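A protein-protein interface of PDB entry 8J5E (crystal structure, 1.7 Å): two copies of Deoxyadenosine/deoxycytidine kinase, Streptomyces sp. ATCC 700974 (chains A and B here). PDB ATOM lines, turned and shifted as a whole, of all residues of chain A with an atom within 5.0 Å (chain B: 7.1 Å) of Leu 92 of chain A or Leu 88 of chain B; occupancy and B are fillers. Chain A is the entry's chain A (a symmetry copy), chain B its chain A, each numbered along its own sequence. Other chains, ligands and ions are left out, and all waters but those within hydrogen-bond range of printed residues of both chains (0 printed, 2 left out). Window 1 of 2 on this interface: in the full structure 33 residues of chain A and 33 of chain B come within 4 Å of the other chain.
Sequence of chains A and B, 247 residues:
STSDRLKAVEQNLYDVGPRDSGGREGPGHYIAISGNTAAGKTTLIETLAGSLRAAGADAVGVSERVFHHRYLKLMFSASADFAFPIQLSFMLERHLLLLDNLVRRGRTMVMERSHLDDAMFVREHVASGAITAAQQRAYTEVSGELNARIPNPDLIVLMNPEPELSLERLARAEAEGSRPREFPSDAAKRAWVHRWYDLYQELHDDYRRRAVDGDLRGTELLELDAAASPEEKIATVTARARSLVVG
A ring nitrogen (NE2) of His 69 of chain B lies within hydrogen-bond range of the side-chain carboxylate (OE1) of Glu 93 of chain A (2.9 Å).
ND1 of His 95 of chain A lies close to O of Leu 146 of chain A (3.4 Å).
Ser 89 of chain A touches Leu 92 of chain B. Leu 92 of chain A touches Leu 88 of chain B (CD2 to C, 3.7 Å). CD2 of His 95 of chain A touches CB of Pro 85 of chain B, 3.8 Å away. CD1 of Leu 96 of chain A touches NE2 of His 69 of chain B (3.6 Å). CD2 of Leu 96 of chain A touches CD2 of Phe 82 of chain B, 3.8 Å away. Pro 85 of chain B touches Leu 96 of chain A (CB to CD2, 3.7 Å). Leu 96 of chain A touches Ile 86 of chain B (CD2 to CD1, 3.7 Å). Val 142 of chain A touches Leu 88 of chain B. Val 142 of chain A touches Ala 138 of chain B (CG2 to O, 3.5 Å). Leu 146 of chain A touches Phe 84 of chain B.
Of chain B, only Pro 85, Leu 88 and Ser 89 come within 4 Å of Leu 92 of chain A. Printed residues of chain A within 4 Å of Leu 88 of chain B: Leu 92 and Val 142. Of the printed residues of chain B, His 95 of chain A touches Pro 85. Printed residues of chain B within 4 Å of Val 142 of chain A: Leu 88 (3.8 Å), Ala 138 (3.5 Å) and Val 142 (3.3 Å). Of the printed residues of chain B, Leu 146 of chain A touches Phe 84. Of the printed residues of chain B, Leu 96 of chain A touches His 69 (3.6 Å), Phe 82 (3.8 Å), Pro 85 (3.7 Å) and Ile 86 (3.7 Å). The nearest residue of chain B that does not touch Leu 92 of chain A is Leu 92 of chain B (4.4 Å). The nearest residue of chain A that does not touch Leu 88 of chain B is Leu 146 of chain A (4.1 Å). The nearest printed residue of chain A that does not touch Phe 82 of chain B is His 95 of chain A (6.4 Å).
Of the 23 printed residues of chain B, 10 touch a printed residue of chain A. Printed residues of chain B that touch a printed residue of chain A: His 69, Phe 82, Phe 84, Pro 85, Ile 86, Leu 88, Ser 89, Leu 92, Ala 138 and Val 142. Hydrophobic or aromatic side chains of chain B within 4 Å of the printed part of chain A: His 69, Phe 82, Phe 84, Pro 85, Ile 86, Leu 88, Leu 92, Ala 138 and Val 142. Hydrophobic or aromatic side chains of chain A within 4 Å of the printed part of chain B: Leu 88, Leu 92, His 95, Leu 96, Val 142 and Leu 146. Along chain A the printed residues that touch a printed residue of chain B span positions 88 to 146. Among the printed residues, 16 pairs touch across the chains.
Leu 88 of chain A touches Leu 92 of chain B, and with the chains exchanged Leu 92 of chain A touches Leu 88 of chain B. Leu 88 of chain A touches Val 142 of chain B, and with the chains exchanged Val 142 of chain A touches Leu 88 of chain B. Ser 89 of chain A touches Leu 92 of chain B, and with the chains exchanged Leu 92 of chain A touches Ser 89 of chain B. Val 142 of chain A touches its own counterpart, Val 142 of chain B. Of the 16 pairs that touch across the chains among the printed residues, 7 have their exchanged pair printed and touching as well.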
ATOM      1  N   LEU A  88     -16.053  14.272 -24.629  1.00  0.00           N
ATOM      2  CA  LEU A  88     -17.449  13.876 -24.832  1.00  0.00           C
ATOM      3  C   LEU A  88     -17.933  14.309 -26.206  1.00  0.00           C
ATOM      4  O   LEU A  88     -18.664  13.576 -26.886  1.00  0.00           O
ATOM      5  CB  LEU A  88     -18.343  14.484 -23.746  1.00  0.00           C
ATOM      6  CG  LEU A  88     -18.221  13.884 -22.349  1.00  0.00           C
ATOM      7  CD1 LEU A  88     -18.964  14.786 -21.344  1.00  0.00           C
ATOM      8  CD2 LEU A  88     -18.801  12.470 -22.344  1.00  0.00           C
ATOM      9  N   SER A  89     -17.509  15.491 -26.644  1.00  0.00           N
ATOM     10  CA  SER A  89     -17.931  16.004 -27.945  1.00  0.00           C
ATOM     11  C   SER A  89     -17.399  15.166 -29.106  1.00  0.00           C
ATOM     12  O   SER A  89     -18.147  14.879 -30.053  1.00  0.00           O
ATOM     13  CB  SER A  89     -17.480  17.455 -28.087  1.00  0.00           C
ATOM     14  OG  SER A  89     -17.874  17.946 -29.355  1.00  0.00           O
ATOM     15  N   PHE A  90     -16.120  14.767 -29.065  1.00  0.00           N
ATOM     16  CA  PHE A  90     -15.594  13.904 -30.127  1.00  0.00           C
ATOM     17  C   PHE A  90     -16.420  12.636 -30.244  1.00  0.00           C
ATOM     18  O   PHE A  90     -16.839  12.243 -31.343  1.00  0.00           O
ATOM     19  CB  PHE A  90     -14.131  13.545 -29.862  1.00  0.00           C
ATOM     20  CG  PHE A  90     -13.138  14.485 -30.520  1.00  0.00           C
ATOM     21  CD1 PHE A  90     -12.922  14.436 -31.885  1.00  0.00           C
ATOM     22  CD2 PHE A  90     -12.406  15.380 -29.764  1.00  0.00           C
ATOM     23  CE1 PHE A  90     -12.004  15.279 -32.494  1.00  0.00           C
ATOM     24  CE2 PHE A  90     -11.485  16.235 -30.370  1.00  0.00           C
ATOM     25  CZ  PHE A  90     -11.285  16.176 -31.731  1.00  0.00           C
ATOM     26  N   MET A  91     -16.627  11.961 -29.117  1.00  0.00           N
ATOM     27  CA  MET A  91     -17.425  10.737 -29.091  1.00  0.00           C
ATOM     28  C   MET A  91     -18.814  10.978 -29.651  1.00  0.00           C
ATOM     29  O   MET A  91     -19.304  10.218 -30.499  1.00  0.00           O
ATOM     30  CB  MET A  91     -17.549  10.246 -27.651  1.00  0.00           C
ATOM     31  CG  MET A  91     -18.615   9.169 -27.480  1.00  0.00           C
ATOM     32  SD  MET A  91     -18.521   8.496 -25.825  1.00  0.00           S
ATOM     33  CE  MET A  91     -19.292   9.816 -24.942  1.00  0.00           C
ATOM     34  N   LEU A  92     -19.469  12.042 -29.178  1.00  0.00           N
ATOM     35  CA  LEU A  92     -20.872  12.249 -29.515  1.00  0.00           C
ATOM     36  C   LEU A  92     -21.043  12.639 -30.974  1.00  0.00           C
ATOM     37  O   LEU A  92     -21.958  12.158 -31.645  1.00  0.00           O
ATOM     38  CB  LEU A  92     -21.463  13.324 -28.604  1.00  0.00           C
ATOM     39  CG  LEU A  92     -22.954  13.534 -28.795  1.00  0.00           C
ATOM     40  CD1 LEU A  92     -23.698  12.249 -28.445  1.00  0.00           C
ATOM     41  CD2 LEU A  92     -23.391  14.669 -27.883  1.00  0.00           C
ATOM     42  N   GLU A  93     -20.197  13.541 -31.478  1.00  0.00           N
ATOM     43  CA  GLU A  93     -20.368  13.958 -32.864  1.00  0.00           C
ATOM     44  C   GLU A  93     -20.052  12.814 -33.809  1.00  0.00           C
ATOM     45  O   GLU A  93     -20.763  12.621 -34.808  1.00  0.00           O
ATOM     46  CB  GLU A  93     -19.505  15.184 -33.169  1.00  0.00           C
ATOM     47  CG  GLU A  93     -19.892  16.387 -32.331  1.00  0.00           C
ATOM     48  CD  GLU A  93     -21.357  16.769 -32.523  1.00  0.00           C
ATOM     49  OE1 GLU A  93     -21.858  16.679 -33.668  1.00  0.00           O
ATOM     50  OE2 GLU A  93     -22.015  17.140 -31.527  1.00  0.00           O
ATOM     51  N   ARG A  94     -19.034  12.012 -33.477  1.00  0.00           N
ATOM     52  CA  ARG A  94     -18.733  10.839 -34.293  1.00  0.00           C
ATOM     53  C   ARG A  94     -19.889   9.858 -34.247  1.00  0.00           C
ATOM     54  O   ARG A  94     -20.289   9.297 -35.281  1.00  0.00           O
ATOM     55  CB  ARG A  94     -17.441  10.171 -33.809  1.00  0.00           C
ATOM     56  CG  ARG A  94     -16.836   9.188 -34.832  1.00  0.00           C
ATOM     57  CD  ARG A  94     -15.735   8.300 -34.213  1.00  0.00           C
ATOM     58  NE  ARG A  94     -14.733   9.074 -33.476  1.00  0.00           N
ATOM     59  CZ  ARG A  94     -13.829   9.870 -34.037  1.00  0.00           C
ATOM     60  NH1 ARG A  94     -13.713   9.976 -35.357  1.00  0.00           N
ATOM     61  NH2 ARG A  94     -13.026  10.593 -33.256  1.00  0.00           N
ATOM     62  N   HIS A  95     -20.457   9.657 -33.054  1.00  0.00           N
ATOM     63  CA  HIS A  95     -21.588   8.749 -32.927  1.00  0.00           C
ATOM     64  C   HIS A  95     -22.742   9.179 -33.825  1.00  0.00           C
ATOM     65  O   HIS A  95     -23.298   8.362 -34.575  1.00  0.00           O
ATOM     66  CB  HIS A  95     -22.030   8.675 -31.469  1.00  0.00           C
ATOM     67  CG  HIS A  95     -23.271   7.876 -31.278  1.00  0.00           C
ATOM     68  ND1 HIS A  95     -23.253   6.509 -31.088  1.00  0.00           N
ATOM     69  CD2 HIS A  95     -24.573   8.247 -31.272  1.00  0.00           C
ATOM     70  CE1 HIS A  95     -24.498   6.077 -30.965  1.00  0.00           C
ATOM     71  NE2 HIS A  95     -25.316   7.111 -31.068  1.00  0.00           N
ATOM     72  N   LEU A  96     -23.117  10.461 -33.763  1.00  0.00           N
ATOM     73  CA  LEU A  96     -24.281  10.922 -34.520  1.00  0.00           C
ATOM     74  C   LEU A  96     -24.029  10.841 -36.016  1.00  0.00           C
ATOM     75  O   LEU A  96     -24.930  10.481 -36.783  1.00  0.00           O
ATOM     76  CB  LEU A  96     -24.630  12.357 -34.125  1.00  0.00           C
ATOM     77  CG  LEU A  96     -25.431  12.479 -32.829  1.00  0.00           C
ATOM     78  CD1 LEU A  96     -25.378  13.887 -32.299  1.00  0.00           C
ATOM     79  CD2 LEU A  96     -26.873  12.082 -33.120  1.00  0.00           C
ATOM     80  N   LEU A  97     -22.806  11.184 -36.451  1.00  0.00           N
ATOM     81  CA  LEU A  97     -22.477  11.084 -37.873  1.00  0.00           C
ATOM     82  C   LEU A  97     -22.624   9.650 -38.368  1.00  0.00           C
ATOM     83  O   LEU A  97     -23.178   9.419 -39.452  1.00  0.00           O
ATOM     84  CB  LEU A  97     -21.055  11.596 -38.141  1.00  0.00           C
ATOM     85  CG  LEU A  97     -20.793  12.176 -39.543  1.00  0.00           C
ATOM     86  CD1 LEU A  97     -21.779  13.288 -39.890  1.00  0.00           C
ATOM     87  CD2 LEU A  97     -19.367  12.630 -39.798  1.00  0.00           C
ATOM     88  N   VAL A 142     -21.550   6.304 -20.612  1.00  0.00           N
ATOM     89  CA  VAL A 142     -22.187   6.823 -21.824  1.00  0.00           C
ATOM     90  C   VAL A 142     -21.595   6.178 -23.070  1.00  0.00           C
ATOM     91  O   VAL A 142     -22.323   5.811 -24.003  1.00  0.00           O
ATOM     92  CB  VAL A 142     -22.072   8.353 -21.890  1.00  0.00           C
ATOM     93  CG1 VAL A 142     -22.492   8.843 -23.288  1.00  0.00           C
ATOM     94  CG2 VAL A 142     -22.982   8.953 -20.870  1.00  0.00           C
ATOM     95  N   LEU A 146     -23.572   4.288 -26.120  1.00  0.00           N
ATOM     96  CA  LEU A 146     -23.504   4.777 -27.495  1.00  0.00           C
ATOM     97  C   LEU A 146     -22.914   3.724 -28.426  1.00  0.00           C
ATOM     98  O   LEU A 146     -23.443   3.470 -29.517  1.00  0.00           O
ATOM     99  CB  LEU A 146     -22.670   6.059 -27.559  1.00  0.00           C
ATOM    100  CG  LEU A 146     -23.280   7.290 -26.888  1.00  0.00           C
ATOM    101  CD1 LEU A 146     -22.289   8.456 -27.007  1.00  0.00           C
ATOM    102  CD2 LEU A 146     -24.627   7.660 -27.508  1.00  0.00           C
ATOM    103  N   HIS B  69     -28.964  20.794 -32.729  1.00  0.00           N
ATOM    104  CA  HIS B  69     -28.095  20.007 -33.580  1.00  0.00           C
ATOM    105  C   HIS B  69     -28.648  19.991 -35.000  1.00  0.00           C
ATOM    106  O   HIS B  69     -29.858  20.111 -35.228  1.00  0.00           O
ATOM    107  CB  HIS B  69     -27.956  18.580 -33.034  1.00  0.00           C
ATOM    108  CG  HIS B  69     -26.716  17.888 -33.500  1.00  0.00           C
ATOM    109  ND1 HIS B  69     -26.656  17.201 -34.695  1.00  0.00           N
ATOM    110  CD2 HIS B  69     -25.471  17.828 -32.967  1.00  0.00           C
ATOM    111  CE1 HIS B  69     -25.432  16.729 -34.866  1.00  0.00           C
ATOM    112  NE2 HIS B  69     -24.692  17.095 -33.833  1.00  0.00           N
ATOM    113  N   PHE B  82     -32.491   8.514 -31.939  1.00  0.00           N
ATOM    114  CA  PHE B  82     -31.746   9.762 -31.864  1.00  0.00           C
ATOM    115  C   PHE B  82     -32.014  10.593 -30.622  1.00  0.00           C
ATOM    116  O   PHE B  82     -31.274  11.555 -30.380  1.00  0.00           O
ATOM    117  CB  PHE B  82     -32.025  10.618 -33.108  1.00  0.00           C
ATOM    118  CG  PHE B  82     -31.262  10.151 -34.304  1.00  0.00           C
ATOM    119  CD1 PHE B  82     -31.733   9.085 -35.058  1.00  0.00           C
ATOM    120  CD2 PHE B  82     -30.038  10.710 -34.628  1.00  0.00           C
ATOM    121  CE1 PHE B  82     -31.016   8.617 -36.137  1.00  0.00           C
ATOM    122  CE2 PHE B  82     -29.311  10.236 -35.712  1.00  0.00           C
ATOM    123  CZ  PHE B  82     -29.804   9.193 -36.456  1.00  0.00           C
ATOM    124  N   ALA B  83     -33.060  10.298 -29.850  1.00  0.00           N
ATOM    125  CA  ALA B  83     -33.357  11.173 -28.716  1.00  0.00           C
ATOM    126  C   ALA B  83     -32.223  11.167 -27.684  1.00  0.00           C
ATOM    127  O   ALA B  83     -31.881  12.221 -27.129  1.00  0.00           O
ATOM    128  CB  ALA B  83     -34.692  10.790 -28.075  1.00  0.00           C
ATOM    129  N   PHE B  84     -31.627   9.996 -27.403  1.00  0.00           N
ATOM    130  CA  PHE B  84     -30.533   9.957 -26.428  1.00  0.00           C
ATOM    131  C   PHE B  84     -29.324  10.776 -26.869  1.00  0.00           C
ATOM    132  O   PHE B  84     -28.904  11.678 -26.116  1.00  0.00           O
ATOM    133  CB  PHE B  84     -30.185   8.496 -26.116  1.00  0.00           C
ATOM    134  CG  PHE B  84     -29.036   8.312 -25.164  1.00  0.00           C
ATOM    135  CD1 PHE B  84     -29.069   8.847 -23.884  1.00  0.00           C
ATOM    136  CD2 PHE B  84     -27.926   7.557 -25.546  1.00  0.00           C
ATOM    137  CE1 PHE B  84     -28.011   8.661 -22.999  1.00  0.00           C
ATOM    138  CE2 PHE B  84     -26.865   7.358 -24.662  1.00  0.00           C
ATOM    139  CZ  PHE B  84     -26.917   7.902 -23.381  1.00  0.00           C
ATOM    140  N   PRO B  85     -28.729  10.552 -28.051  1.00  0.00           N
ATOM    141  CA  PRO B  85     -27.556  11.366 -28.408  1.00  0.00           C
ATOM    142  C   PRO B  85     -27.892  12.831 -28.614  1.00  0.00           C
ATOM    143  O   PRO B  85     -27.058  13.691 -28.301  1.00  0.00           O
ATOM    144  CB  PRO B  85     -27.031  10.709 -29.693  1.00  0.00           C
ATOM    145  CG  PRO B  85     -28.236   9.937 -30.250  1.00  0.00           C
ATOM    146  CD  PRO B  85     -28.986   9.485 -29.048  1.00  0.00           C
ATOM    147  N   ILE B  86     -29.089  13.156 -29.112  1.00  0.00           N
ATOM    148  CA  ILE B  86     -29.408  14.567 -29.294  1.00  0.00           C
ATOM    149  C   ILE B  86     -29.613  15.245 -27.944  1.00  0.00           C
ATOM    150  O   ILE B  86     -29.208  16.394 -27.751  1.00  0.00           O
ATOM    151  CB  ILE B  86     -30.612  14.752 -30.245  1.00  0.00           C
ATOM    152  CG1 ILE B  86     -30.263  14.268 -31.653  1.00  0.00           C
ATOM    153  CG2 ILE B  86     -30.935  16.239 -30.384  1.00  0.00           C
ATOM    154  CD1 ILE B  86     -29.047  14.953 -32.246  1.00  0.00           C
ATOM    155  N   GLN B  87     -30.197  14.539 -26.964  1.00  0.00           N
ATOM    156  CA  GLN B  87     -30.268  15.137 -25.631  1.00  0.00           C
ATOM    157  C   GLN B  87     -28.869  15.322 -25.036  1.00  0.00           C
ATOM    158  O   GLN B  87     -28.607  16.329 -24.367  1.00  0.00           O
ATOM    159  CB  GLN B  87     -31.141  14.286 -24.711  1.00  0.00           C
ATOM    160  CG  GLN B  87     -32.671  14.472 -24.929  1.00  0.00           C
ATOM    161  CD  GLN B  87     -33.144  15.923 -24.805  1.00  0.00           C
ATOM    162  OE1 GLN B  87     -34.003  16.396 -25.582  1.00  0.00           O
ATOM    163  NE2 GLN B  87     -32.604  16.629 -23.829  1.00  0.00           N
ATOM    164  N   LEU B  88     -27.970  14.354 -25.238  1.00  0.00           N
ATOM    165  CA  LEU B  88     -26.588  14.548 -24.792  1.00  0.00           C
ATOM    166  C   LEU B  88     -25.990  15.790 -25.430  1.00  0.00           C
ATOM    167  O   LEU B  88     -25.257  16.551 -24.782  1.00  0.00           O
ATOM    168  CB  LEU B  88     -25.736  13.321 -25.135  1.00  0.00           C
ATOM    169  CG  LEU B  88     -25.985  12.065 -24.305  1.00  0.00           C
ATOM    170  CD1 LEU B  88     -25.261  10.874 -24.961  1.00  0.00           C
ATOM    171  CD2 LEU B  88     -25.487  12.286 -22.877  1.00  0.00           C
ATOM    172  N   SER B  89     -26.317  16.029 -26.697  1.00  0.00           N
ATOM    173  CA  SER B  89     -25.781  17.189 -27.404  1.00  0.00           C
ATOM    174  C   SER B  89     -26.279  18.511 -26.824  1.00  0.00           C
ATOM    175  O   SER B  89     -25.487  19.451 -26.661  1.00  0.00           O
ATOM    176  CB  SER B  89     -26.140  17.089 -28.884  1.00  0.00           C
ATOM    177  OG  SER B  89     -25.635  18.222 -29.566  1.00  0.00           O
ATOM    178  N   PHE B  90     -27.579  18.615 -26.512  1.00  0.00           N
ATOM    179  CA  PHE B  90     -28.080  19.844 -25.889  1.00  0.00           C
ATOM    180  C   PHE B  90     -27.320  20.144 -24.609  1.00  0.00           C
ATOM    181  O   PHE B  90     -26.851  21.271 -24.392  1.00  0.00           O
ATOM    182  CB  PHE B  90     -29.575  19.731 -25.587  1.00  0.00           C
ATOM    183  CG  PHE B  90     -30.468  20.261 -26.694  1.00  0.00           C
ATOM    184  CD1 PHE B  90     -30.595  21.622 -26.903  1.00  0.00           C
ATOM    185  CD2 PHE B  90     -31.197  19.397 -27.486  1.00  0.00           C
ATOM    186  CE1 PHE B  90     -31.421  22.118 -27.902  1.00  0.00           C
ATOM    187  CE2 PHE B  90     -32.026  19.887 -28.495  1.00  0.00           C
ATOM    188  CZ  PHE B  90     -32.138  21.245 -28.694  1.00  0.00           C
ATOM    189  N   MET B  91     -27.227  19.149 -23.732  1.00  0.00           N
ATOM    190  CA  MET B  91     -26.502  19.302 -22.472  1.00  0.00           C
ATOM    191  C   MET B  91     -25.067  19.731 -22.716  1.00  0.00           C
ATOM    192  O   MET B  91     -24.564  20.674 -22.088  1.00  0.00           O
ATOM    193  CB  MET B  91     -26.502  17.971 -21.725  1.00  0.00           C
ATOM    194  CG  MET B  91     -25.512  17.940 -20.566  1.00  0.00           C
ATOM    195  SD  MET B  91     -25.754  16.443 -19.616  1.00  0.00           S
ATOM    196  CE  MET B  91     -24.971  15.293 -20.702  1.00  0.00           C
ATOM    197  N   LEU B  92     -24.387  19.036 -23.632  1.00  0.00           N
ATOM    198  CA  LEU B  92     -22.955  19.251 -23.801  1.00  0.00           C
ATOM    199  C   LEU B  92     -22.666  20.602 -24.433  1.00  0.00           C
ATOM    200  O   LEU B  92     -21.735  21.297 -24.020  1.00  0.00           O
ATOM    201  CB  LEU B  92     -22.367  18.127 -24.655  1.00  0.00           C
ATOM    202  CG  LEU B  92     -20.857  18.194 -24.795  1.00  0.00           C
ATOM    203  CD1 LEU B  92     -20.212  18.042 -23.421  1.00  0.00           C
ATOM    204  CD2 LEU B  92     -20.421  17.066 -25.717  1.00  0.00           C
ATOM    205  N   GLU B  93     -23.424  20.980 -25.465  1.00  0.00           N
ATOM    206  CA  GLU B  93     -23.138  22.255 -26.110  1.00  0.00           C
ATOM    207  C   GLU B  93     -23.453  23.409 -25.177  1.00  0.00           C
ATOM    208  O   GLU B  93     -22.689  24.385 -25.118  1.00  0.00           O
ATOM    209  CB  GLU B  93     -23.908  22.379 -27.426  1.00  0.00           C
ATOM    210  CG  GLU B  93     -23.512  21.315 -28.432  1.00  0.00           C
ATOM    211  CD  GLU B  93     -22.019  21.353 -28.743  1.00  0.00           C
ATOM    212  OE1 GLU B  93     -21.448  22.465 -28.825  1.00  0.00           O
ATOM    213  OE2 GLU B  93     -21.409  20.271 -28.885  1.00  0.00           O
ATOM    214  N   ARG B  94     -24.535  23.285 -24.398  1.00  0.00           N
ATOM    215  CA  ARG B  94     -24.844  24.317 -23.413  1.00  0.00           C
ATOM    216  C   ARG B  94     -23.751  24.386 -22.365  1.00  0.00           C
ATOM    217  O   ARG B  94     -23.314  25.481 -21.972  1.00  0.00           O
ATOM    218  CB  ARG B  94     -26.201  24.036 -22.758  1.00  0.00           C
ATOM    219  CG  ARG B  94     -26.790  25.253 -22.016  1.00  0.00           C
ATOM    220  CD  ARG B  94     -27.978  24.869 -21.107  1.00  0.00           C
ATOM    221  NE  ARG B  94     -28.983  24.060 -21.803  1.00  0.00           N
ATOM    222  CZ  ARG B  94     -29.801  24.516 -22.745  1.00  0.00           C
ATOM    223  NH1 ARG B  94     -29.822  25.799 -23.092  1.00  0.00           N
ATOM    224  NH2 ARG B  94     -30.613  23.663 -23.369  1.00  0.00           N
ATOM    225  N   VAL B 122     -34.992  14.785 -21.051  1.00  0.00           N
ATOM    226  CA  VAL B 122     -34.690  13.363 -20.996  1.00  0.00           C
ATOM    227  C   VAL B 122     -35.827  12.604 -20.319  1.00  0.00           C
ATOM    228  O   VAL B 122     -36.241  11.538 -20.792  1.00  0.00           O
ATOM    229  CB  VAL B 122     -33.343  13.149 -20.282  1.00  0.00           C
ATOM    230  CG1 VAL B 122     -33.090  11.665 -20.066  1.00  0.00           C
ATOM    231  CG2 VAL B 122     -32.264  13.736 -21.127  1.00  0.00           C
ATOM    232  N   ILE B 131     -36.012   6.820 -24.818  1.00  0.00           N
ATOM    233  CA  ILE B 131     -34.742   6.658 -24.116  1.00  0.00           C
ATOM    234  C   ILE B 131     -34.926   5.575 -23.059  1.00  0.00           C
ATOM    235  O   ILE B 131     -35.901   5.608 -22.299  1.00  0.00           O
ATOM    236  CB  ILE B 131     -34.283   7.988 -23.493  1.00  0.00           C
ATOM    237  CG1 ILE B 131     -33.966   9.006 -24.602  1.00  0.00           C
ATOM    238  CG2 ILE B 131     -33.058   7.780 -22.575  1.00  0.00           C
ATOM    239  CD1 ILE B 131     -33.437  10.370 -24.084  1.00  0.00           C
ATOM    240  N   GLN B 135     -29.925   4.110 -20.573  1.00  0.00           N
ATOM    241  CA  GLN B 135     -29.450   5.350 -21.183  1.00  0.00           C
ATOM    242  C   GLN B 135     -29.643   6.521 -20.236  1.00  0.00           C
ATOM    243  O   GLN B 135     -28.749   7.359 -20.080  1.00  0.00           O
ATOM    244  CB  GLN B 135     -30.189   5.601 -22.503  1.00  0.00           C
ATOM    245  CG  GLN B 135     -29.641   4.785 -23.669  1.00  0.00           C
ATOM    246  CD  GLN B 135     -30.538   4.858 -24.902  1.00  0.00           C
ATOM    247  OE1 GLN B 135     -31.756   4.969 -24.794  1.00  0.00           O
ATOM    248  NE2 GLN B 135     -29.930   4.793 -26.081  1.00  0.00           N
ATOM    249  N   ALA B 138     -26.944   6.587 -17.576  1.00  0.00           N
ATOM    250  CA  ALA B 138     -25.667   7.088 -18.090  1.00  0.00           C
ATOM    251  C   ALA B 138     -25.708   8.601 -18.268  1.00  0.00           C
ATOM    252  O   ALA B 138     -24.764   9.308 -17.881  1.00  0.00           O
ATOM    253  CB  ALA B 138     -25.331   6.407 -19.424  1.00  0.00           C
ATOM    254  N   TYR B 139     -26.812   9.113 -18.819  1.00  0.00           N
ATOM    255  CA  TYR B 139     -27.001  10.559 -18.923  1.00  0.00           C
ATOM    256  C   TYR B 139     -26.864  11.231 -17.566  1.00  0.00           C
ATOM    257  O   TYR B 139     -26.179  12.254 -17.433  1.00  0.00           O
ATOM    258  CB  TYR B 139     -28.378  10.863 -19.525  1.00  0.00           C
ATOM    259  CG  TYR B 139     -28.720  12.336 -19.621  1.00  0.00           C
ATOM    260  CD1 TYR B 139     -29.270  13.010 -18.538  1.00  0.00           C
ATOM    261  CD2 TYR B 139     -28.495  13.053 -20.796  1.00  0.00           C
ATOM    262  CE1 TYR B 139     -29.593  14.346 -18.607  1.00  0.00           C
ATOM    263  CE2 TYR B 139     -28.825  14.402 -20.876  1.00  0.00           C
ATOM    264  CZ  TYR B 139     -29.366  15.040 -19.780  1.00  0.00           C
ATOM    265  OH  TYR B 139     -29.704  16.384 -19.843  1.00  0.00           O
ATOM    266  N   THR B 140     -27.517  10.665 -16.544  1.00  0.00           N
ATOM    267  CA  THR B 140     -27.515  11.286 -15.221  1.00  0.00           C
ATOM    268  C   THR B 140     -26.108  11.349 -14.638  1.00  0.00           C
ATOM    269  O   THR B 140     -25.742  12.342 -13.999  1.00  0.00           O
ATOM    270  CB  THR B 140     -28.478  10.528 -14.299  1.00  0.00           C
ATOM    271  OG1 THR B 140     -29.817  10.673 -14.814  1.00  0.00           O
ATOM    272  CG2 THR B 140     -28.433  11.084 -12.881  1.00  0.00           C
ATOM    273  N   VAL B 142     -23.208  11.557 -16.331  1.00  0.00           N
ATOM    274  CA  VAL B 142     -22.463  12.616 -17.014  1.00  0.00           C
ATOM    275  C   VAL B 142     -23.005  13.990 -16.643  1.00  0.00           C
ATOM    276  O   VAL B 142     -22.238  14.932 -16.401  1.00  0.00           O
ATOM    277  CB  VAL B 142     -22.488  12.409 -18.535  1.00  0.00           C
ATOM    278  CG1 VAL B 142     -21.949  13.668 -19.238  1.00  0.00           C
ATOM    279  CG2 VAL B 142     -21.617  11.247 -18.881  1.00  0.00           C
ATOM    280  N   SER B 143     -24.331  14.122 -16.595  1.00  0.00           N
ATOM    281  CA  SER B 143     -24.949  15.391 -16.217  1.00  0.00           C
ATOM    282  C   SER B 143     -24.467  15.851 -14.846  1.00  0.00           C
ATOM    283  O   SER B 143     -24.156  17.036 -14.649  1.00  0.00           O
ATOM    284  CB  SER B 143     -26.478  15.242 -16.227  1.00  0.00           C
ATOM    285  OG  SER B 143     -27.118  16.463 -15.877  1.00  0.00           O
ATOM    286  N   LEU B 146     -20.937  17.218 -15.199  1.00  0.00           N
ATOM    287  CA  LEU B 146     -20.885  18.483 -15.930  1.00  0.00           C
ATOM    288  C   LEU B 146     -21.469  19.622 -15.102  1.00  0.00           C
ATOM    289  O   LEU B 146     -20.884  20.710 -15.012  1.00  0.00           O
ATOM    290  CB  LEU B 146     -21.640  18.359 -17.255  1.00  0.00           C
ATOM    291  CG  LEU B 146     -21.009  17.442 -18.303  1.00  0.00           C
ATOM    292  CD1 LEU B 146     -21.923  17.401 -19.535  1.00  0.00           C
ATOM    293  CD2 LEU B 146     -19.605  17.907 -18.687  1.00  0.00           C
